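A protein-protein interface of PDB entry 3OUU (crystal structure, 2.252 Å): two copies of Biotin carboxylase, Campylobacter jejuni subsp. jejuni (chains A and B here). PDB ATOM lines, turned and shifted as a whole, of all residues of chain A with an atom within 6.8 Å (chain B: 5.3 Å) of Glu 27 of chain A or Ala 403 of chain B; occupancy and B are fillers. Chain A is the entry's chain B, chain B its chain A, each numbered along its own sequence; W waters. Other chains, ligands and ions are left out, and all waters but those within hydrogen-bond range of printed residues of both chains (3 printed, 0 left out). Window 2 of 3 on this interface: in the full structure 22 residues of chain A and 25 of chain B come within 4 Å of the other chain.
Among the printed residues, pairs that only touch across the chains: Lys 26 of chain A with Val 407 of chain B (3.9 Å), Glu 27 of chain A with Ala 403 of chain B (3.9 Å) and Glu 27 of chain A with Val 407 of chain B (3.8 Å).
No position is printed for both chains.
Of the 5 pairs that touch across the chains among the printed residues, none has its exchanged pair printed and touching as well.
Printed residues of chain B that touch a printed residue of chain A: Arg 366, Ala 403, Lys 404 and Val 407.
Hydrophobic or aromatic side chains of chain B within 4 Å of the printed part of chain A: Ala 403 and Val 407.
Among the printed residues, Asp or Glu carboxylates within 4 Å of a Lys or Arg side-chain nitrogen of the other chain: Glu 27 of chain A with Lys 404 of chain B (3.0 Å) and Asp 311 of chain A with Arg 366 of chain B (3.9 Å).
The side-chain amino group (NZ) of Lys 404 of chain B is in salt-bridge range of the side-chain carboxylate (OE2) of Glu 27 of chain A (3.0 Å).
The guanidinium group of Arg 366 of chain B lies within salt-bridge range of the side-chain carboxylate of Asp 311 of chain A.
The side-chain hydroxyl (OG1) of Thr 24 of chain A is in hydrogen-bond range of the side-chain carboxylate (OD2) of Asp 311 of chain A, 2.7 Å away.
The backbone carbonyl oxygen of Arg 366 of chain B sits at hydrogen-bond distance from the side-chain amino group of Lys 404 of chain B (2.7 Å).
Water W1 bridges OE1 of Glu 27 of chain A and NZ of Lys 404 of chain B.
Water W3 lies within hydrogen-bond range of NH1 of Arg 366 of chain B (2.6 Å), NZ of Lys 404 of chain B (3.0 Å), OE2 of Glu 27 of chain A (3.0 Å) and OD2 of Asp 311 of chain A (3.2 Å).
Water W2 lies within hydrogen-bond range of the side-chain carboxylate (OE1) of Glu 27 of chain A (2.9 Å) and the backbone carbonyl oxygen (O) of Lys 404 of chain B (3.2 Å).
Of the printed residues of chain B, Glu 27 of chain A touches Ala 403 (3.9 Å), Lys 404 (3.0 Å) and Val 407 (3.8 Å).
Ala 403 of chain B touches just one residue of chain A: Glu 27.
Of the printed residues of chain B, Lys 26 of chain A touches Val 407.
Of the printed residues of chain A, Lys 404 of chain B touches Glu 27.
Of the printed residues of chain A, Val 407 of chain B touches Lys 26 and Glu 27.
Met 28 of chain A touches none of the printed residues of chain B.
Lys 30 of chain A touches none of the printed residues of chain B.
The nearest residue of chain B that does not touch Glu 27 of chain A is Arg 366 of chain B (5.1 Å).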
ATOM      1  N   LEU A  22      -4.086  -0.109   3.606  1.00  0.00           N
ATOM      2  CA  LEU A  22      -2.699   0.103   3.981  1.00  0.00           C
ATOM      3  C   LEU A  22      -2.305  -0.777   5.170  1.00  0.00           C
ATOM      4  O   LEU A  22      -1.308  -1.512   5.116  1.00  0.00           O
ATOM      5  CB  LEU A  22      -2.454   1.573   4.268  1.00  0.00           C
ATOM      6  CG  LEU A  22      -1.038   1.914   4.680  1.00  0.00           C
ATOM      7  CD1 LEU A  22      -0.749   3.273   4.167  1.00  0.00           C
ATOM      8  CD2 LEU A  22      -0.895   1.859   6.201  1.00  0.00           C
ATOM      9  N   ARG A  23      -3.120  -0.744   6.216  1.00  0.00           N
ATOM     10  CA  ARG A  23      -2.843  -1.528   7.409  1.00  0.00           C
ATOM     11  C   ARG A  23      -2.620  -3.009   7.100  1.00  0.00           C
ATOM     12  O   ARG A  23      -1.639  -3.587   7.568  1.00  0.00           O
ATOM     13  CB  ARG A  23      -3.937  -1.352   8.458  1.00  0.00           C
ATOM     14  CG  ARG A  23      -3.803  -0.106   9.259  1.00  0.00           C
ATOM     15  CD  ARG A  23      -5.120   0.204   9.989  1.00  0.00           C
ATOM     16  NE  ARG A  23      -4.959   1.403  10.800  1.00  0.00           N
ATOM     17  CZ  ARG A  23      -5.940   2.208  11.212  1.00  0.00           C
ATOM     18  NH1 ARG A  23      -7.198   1.951  10.884  1.00  0.00           N
ATOM     19  NH2 ARG A  23      -5.647   3.289  11.961  1.00  0.00           N
ATOM     20  N   THR A  24      -3.508  -3.625   6.317  1.00  0.00           N
ATOM     21  CA  THR A  24      -3.359  -5.059   5.982  1.00  0.00           C
ATOM     22  C   THR A  24      -2.093  -5.341   5.137  1.00  0.00           C
ATOM     23  O   THR A  24      -1.343  -6.305   5.379  1.00  0.00           O
ATOM     24  CB  THR A  24      -4.625  -5.614   5.272  1.00  0.00           C
ATOM     25  OG1 THR A  24      -5.659  -5.758   6.232  1.00  0.00           O
ATOM     26  CG2 THR A  24      -4.378  -6.999   4.638  1.00  0.00           C
ATOM     27  N   ILE A  25      -1.867  -4.476   4.156  1.00  0.00           N
ATOM     28  CA  ILE A  25      -0.738  -4.592   3.259  1.00  0.00           C
ATOM     29  C   ILE A  25       0.587  -4.586   4.023  1.00  0.00           C
ATOM     30  O   ILE A  25       1.436  -5.449   3.797  1.00  0.00           O
ATOM     31  CB  ILE A  25      -0.780  -3.527   2.145  1.00  0.00           C
ATOM     32  CG1 ILE A  25      -1.895  -3.873   1.175  1.00  0.00           C
ATOM     33  CG2 ILE A  25       0.539  -3.478   1.405  1.00  0.00           C
ATOM     34  CD1 ILE A  25      -2.437  -2.707   0.384  1.00  0.00           C
ATOM     35  N   LYS A  26       0.726  -3.668   4.967  1.00  0.00           N
ATOM     36  CA  LYS A  26       1.948  -3.552   5.726  1.00  0.00           C
ATOM     37  C   LYS A  26       2.115  -4.697   6.735  1.00  0.00           C
ATOM     38  O   LYS A  26       3.228  -5.154   6.930  1.00  0.00           O
ATOM     39  CB  LYS A  26       2.022  -2.198   6.420  1.00  0.00           C
ATOM     40  CG  LYS A  26       2.062  -1.058   5.440  1.00  0.00           C
ATOM     41  CD  LYS A  26       2.471   0.257   6.102  1.00  0.00           C
ATOM     42  CE  LYS A  26       3.986   0.409   6.137  1.00  0.00           C
ATOM     43  NZ  LYS A  26       4.397   1.620   6.919  1.00  0.00           N
ATOM     44  N   GLU A  27       1.030  -5.163   7.363  1.00  0.00           N
ATOM     45  CA  GLU A  27       1.123  -6.351   8.220  1.00  0.00           C
ATOM     46  C   GLU A  27       1.596  -7.580   7.464  1.00  0.00           C
ATOM     47  O   GLU A  27       2.232  -8.455   8.054  1.00  0.00           O
ATOM     48  CB  GLU A  27      -0.198  -6.693   8.915  1.00  0.00           C
ATOM     49  CG  GLU A  27      -0.496  -5.835  10.102  1.00  0.00           C
ATOM     50  CD  GLU A  27      -1.971  -5.782  10.410  1.00  0.00           C
ATOM     51  OE1 GLU A  27      -2.468  -4.669  10.732  1.00  0.00           O
ATOM     52  OE2 GLU A  27      -2.629  -6.857  10.313  1.00  0.00           O
ATOM     53  N   MET A  28       1.277  -7.669   6.176  1.00  0.00           N
ATOM     54  CA  MET A  28       1.723  -8.833   5.401  1.00  0.00           C
ATOM     55  C   MET A  28       3.157  -8.702   4.934  1.00  0.00           C
ATOM     56  O   MET A  28       3.664  -9.592   4.275  1.00  0.00           O
ATOM     57  CB  MET A  28       0.838  -9.065   4.187  1.00  0.00           C
ATOM     58  CG  MET A  28      -0.629  -9.254   4.529  1.00  0.00           C
ATOM     59  SD  MET A  28      -1.635  -9.421   2.863  1.00  0.00           S
ATOM     60  CE  MET A  28      -1.143 -11.308   2.495  1.00  0.00           C
ATOM     61  N   GLY A  29       3.794  -7.575   5.240  1.00  0.00           N
ATOM     62  CA  GLY A  29       5.161  -7.334   4.813  1.00  0.00           C
ATOM     63  C   GLY A  29       5.301  -6.848   3.372  1.00  0.00           C
ATOM     64  O   GLY A  29       6.391  -6.840   2.819  1.00  0.00           O
ATOM     65  N   LYS A  30       4.206  -6.429   2.754  1.00  0.00           N
ATOM     66  CA  LYS A  30       4.286  -5.927   1.396  1.00  0.00           C
ATOM     67  C   LYS A  30       4.416  -4.419   1.459  1.00  0.00           C
ATOM     68  O   LYS A  30       4.166  -3.838   2.506  1.00  0.00           O
ATOM     69  CB  LYS A  30       3.063  -6.396   0.619  1.00  0.00           C
ATOM     70  CG  LYS A  30       2.976  -7.942   0.626  1.00  0.00           C
ATOM     71  CD  LYS A  30       1.776  -8.474  -0.130  1.00  0.00           C
ATOM     72  CE  LYS A  30       1.623  -9.980   0.089  1.00  0.00           C
ATOM     73  NZ  LYS A  30       2.820 -10.746  -0.350  1.00  0.00           N
ATOM     74  N   ASP A 311      -9.590 -11.702   7.636  1.00  0.00           N
ATOM     75  CA  ASP A 311      -9.209 -10.434   7.024  1.00  0.00           C
ATOM     76  C   ASP A 311      -9.502 -10.562   5.523  1.00  0.00           C
ATOM     77  O   ASP A 311      -8.772 -11.214   4.785  1.00  0.00           O
ATOM     78  CB  ASP A 311      -7.725 -10.127   7.272  1.00  0.00           C
ATOM     79  CG  ASP A 311      -7.318  -8.723   6.764  1.00  0.00           C
ATOM     80  OD1 ASP A 311      -7.983  -8.187   5.843  1.00  0.00           O
ATOM     81  OD2 ASP A 311      -6.331  -8.152   7.288  1.00  0.00           O
ATOM     82  N   ARG B 366      -8.120  -3.774  12.730  1.00  0.00           N
ATOM     83  CA  ARG B 366      -8.530  -5.095  13.109  1.00  0.00           C
ATOM     84  C   ARG B 366      -7.656  -5.642  14.268  1.00  0.00           C
ATOM     85  O   ARG B 366      -6.432  -5.698  14.150  1.00  0.00           O
ATOM     86  CB  ARG B 366      -8.385  -5.976  11.868  1.00  0.00           C
ATOM     87  CG  ARG B 366      -8.963  -7.333  12.015  1.00  0.00           C
ATOM     88  CD  ARG B 366      -9.021  -8.051  10.684  1.00  0.00           C
ATOM     89  NE  ARG B 366      -9.068  -9.473  10.961  1.00  0.00           N
ATOM     90  CZ  ARG B 366      -7.991 -10.238  11.052  1.00  0.00           C
ATOM     91  NH1 ARG B 366      -6.795  -9.706  10.847  1.00  0.00           N
ATOM     92  NH2 ARG B 366      -8.113 -11.532  11.328  1.00  0.00           N
ATOM     93  N   ARG B 398       2.301 -16.035  16.888  1.00  0.00           N
ATOM     94  CA  ARG B 398       3.214 -15.072  17.499  1.00  0.00           C
ATOM     95  C   ARG B 398       3.863 -14.114  16.480  1.00  0.00           C
ATOM     96  O   ARG B 398       3.839 -12.882  16.657  1.00  0.00           O
ATOM     97  CB  ARG B 398       4.289 -15.759  18.329  1.00  0.00           C
ATOM     98  CG  ARG B 398       5.033 -14.766  19.233  1.00  0.00           C
ATOM     99  CD  ARG B 398       5.983 -15.488  20.147  1.00  0.00           C
ATOM    100  NE  ARG B 398       6.651 -14.593  21.080  1.00  0.00           N
ATOM    101  CZ  ARG B 398       7.896 -14.143  20.935  1.00  0.00           C
ATOM    102  NH1 ARG B 398       8.630 -14.502  19.880  1.00  0.00           N
ATOM    103  NH2 ARG B 398       8.410 -13.346  21.869  1.00  0.00           N
ATOM    104  N   ASN B 399       4.401 -14.675  15.399  1.00  0.00           N
ATOM    105  CA  ASN B 399       5.056 -13.859  14.384  1.00  0.00           C
ATOM    106  C   ASN B 399       4.097 -12.883  13.745  1.00  0.00           C
ATOM    107  O   ASN B 399       4.481 -11.776  13.420  1.00  0.00           O
ATOM    108  CB  ASN B 399       5.710 -14.727  13.311  1.00  0.00           C
ATOM    109  CG  ASN B 399       6.976 -15.390  13.805  1.00  0.00           C
ATOM    110  OD1 ASN B 399       7.621 -14.901  14.738  1.00  0.00           O
ATOM    111  ND2 ASN B 399       7.338 -16.512  13.192  1.00  0.00           N
ATOM    112  N   LYS B 400       2.840 -13.282  13.588  1.00  0.00           N
ATOM    113  CA  LYS B 400       1.861 -12.379  13.012  1.00  0.00           C
ATOM    114  C   LYS B 400       1.497 -11.283  14.010  1.00  0.00           C
ATOM    115  O   LYS B 400       1.250 -10.142  13.621  1.00  0.00           O
ATOM    116  CB  LYS B 400       0.613 -13.126  12.533  1.00  0.00           C
ATOM    117  CG  LYS B 400       0.820 -13.824  11.207  1.00  0.00           C
ATOM    118  CD  LYS B 400      -0.394 -14.725  10.918  1.00  0.00           C
ATOM    119  CE  LYS B 400      -0.020 -15.881  10.020  1.00  0.00           C
ATOM    120  NZ  LYS B 400      -0.390 -15.576   8.637  1.00  0.00           N
ATOM    121  N   ALA B 401       1.491 -11.621  15.293  1.00  0.00           N
ATOM    122  CA  ALA B 401       1.175 -10.623  16.303  1.00  0.00           C
ATOM    123  C   ALA B 401       2.306  -9.595  16.399  1.00  0.00           C
ATOM    124  O   ALA B 401       2.046  -8.400  16.609  1.00  0.00           O
ATOM    125  CB  ALA B 401       0.913 -11.272  17.670  1.00  0.00           C
ATOM    126  N   ILE B 402       3.547 -10.059  16.233  1.00  0.00           N
ATOM    127  CA  ILE B 402       4.702  -9.175  16.289  1.00  0.00           C
ATOM    128  C   ILE B 402       4.673  -8.228  15.091  1.00  0.00           C
ATOM    129  O   ILE B 402       4.843  -7.011  15.253  1.00  0.00           O
ATOM    130  CB  ILE B 402       6.025  -9.963  16.307  1.00  0.00           C
ATOM    131  CG1 ILE B 402       6.217 -10.656  17.656  1.00  0.00           C
ATOM    132  CG2 ILE B 402       7.201  -9.061  16.020  1.00  0.00           C
ATOM    133  CD1 ILE B 402       7.278 -11.729  17.589  1.00  0.00           C
ATOM    134  N   ALA B 403       4.423  -8.765  13.893  1.00  0.00           N
ATOM    135  CA  ALA B 403       4.286  -7.885  12.738  1.00  0.00           C
ATOM    136  C   ALA B 403       3.107  -6.890  12.892  1.00  0.00           C
ATOM    137  O   ALA B 403       3.133  -5.813  12.334  1.00  0.00           O
ATOM    138  CB  ALA B 403       4.132  -8.695  11.454  1.00  0.00           C
ATOM    139  N   LYS B 404       2.058  -7.265  13.622  1.00  0.00           N
ATOM    140  CA  LYS B 404       0.924  -6.373  13.777  1.00  0.00           C
ATOM    141  C   LYS B 404       1.287  -5.261  14.782  1.00  0.00           C
ATOM    142  O   LYS B 404       0.920  -4.104  14.589  1.00  0.00           O
ATOM    143  CB  LYS B 404      -0.356  -7.145  14.191  1.00  0.00           C
ATOM    144  CG  LYS B 404      -1.562  -6.261  14.315  1.00  0.00           C
ATOM    145  CD  LYS B 404      -2.815  -6.997  14.778  1.00  0.00           C
ATOM    146  CE  LYS B 404      -3.607  -7.561  13.632  1.00  0.00           C
ATOM    147  NZ  LYS B 404      -4.192  -6.467  12.818  1.00  0.00           N
ATOM    148  N   MET B 405       1.999  -5.638  15.846  1.00  0.00           N
ATOM    149  CA  MET B 405       2.524  -4.698  16.844  1.00  0.00           C
ATOM    150  C   MET B 405       3.364  -3.601  16.175  1.00  0.00           C
ATOM    151  O   MET B 405       3.134  -2.413  16.433  1.00  0.00           O
ATOM    152  CB  MET B 405       3.312  -5.441  17.956  1.00  0.00           C
ATOM    153  CG  MET B 405       3.688  -4.602  19.255  1.00  0.00           C
ATOM    154  SD  MET B 405       2.204  -3.472  19.912  1.00  0.00           S
ATOM    155  CE  MET B 405       1.393  -4.813  21.112  1.00  0.00           C
ATOM    156  N   LYS B 406       4.296  -3.986  15.296  1.00  0.00           N
ATOM    157  CA  LYS B 406       5.131  -3.025  14.567  1.00  0.00           C
ATOM    158  C   LYS B 406       4.305  -1.988  13.789  1.00  0.00           C
ATOM    159  O   LYS B 406       4.643  -0.799  13.802  1.00  0.00           O
ATOM    160  CB  LYS B 406       6.074  -3.702  13.573  1.00  0.00           C
ATOM    161  CG  LYS B 406       6.980  -4.757  14.140  1.00  0.00           C
ATOM    162  CD  LYS B 406       8.321  -4.832  13.397  1.00  0.00           C
ATOM    163  CE  LYS B 406       8.184  -5.115  11.894  1.00  0.00           C
ATOM    164  NZ  LYS B 406       8.099  -6.578  11.543  1.00  0.00           N
ATOM    165  N   VAL B 407       3.268  -2.446  13.076  1.00  0.00           N
ATOM    166  CA  VAL B 407       2.411  -1.544  12.309  1.00  0.00           C
ATOM    167  C   VAL B 407       1.579  -0.659  13.225  1.00  0.00           C
ATOM    168  O   VAL B 407       1.433   0.531  12.972  1.00  0.00           O
ATOM    169  CB  VAL B 407       1.450  -2.297  11.359  1.00  0.00           C
ATOM    170  CG1 VAL B 407       0.404  -1.329  10.768  1.00  0.00           C
ATOM    171  CG2 VAL B 407       2.236  -3.032  10.272  1.00  0.00           C
HETATM  172  O   HOH W   1      -4.372  -3.230  11.730  1.00  0.00           O
HETATM  173  O   HOH W   2      -1.836  -3.286  13.222  1.00  0.00           O
HETATM  174  O   HOH W   3      -5.586  -7.423  10.334  1.00  0.00           O
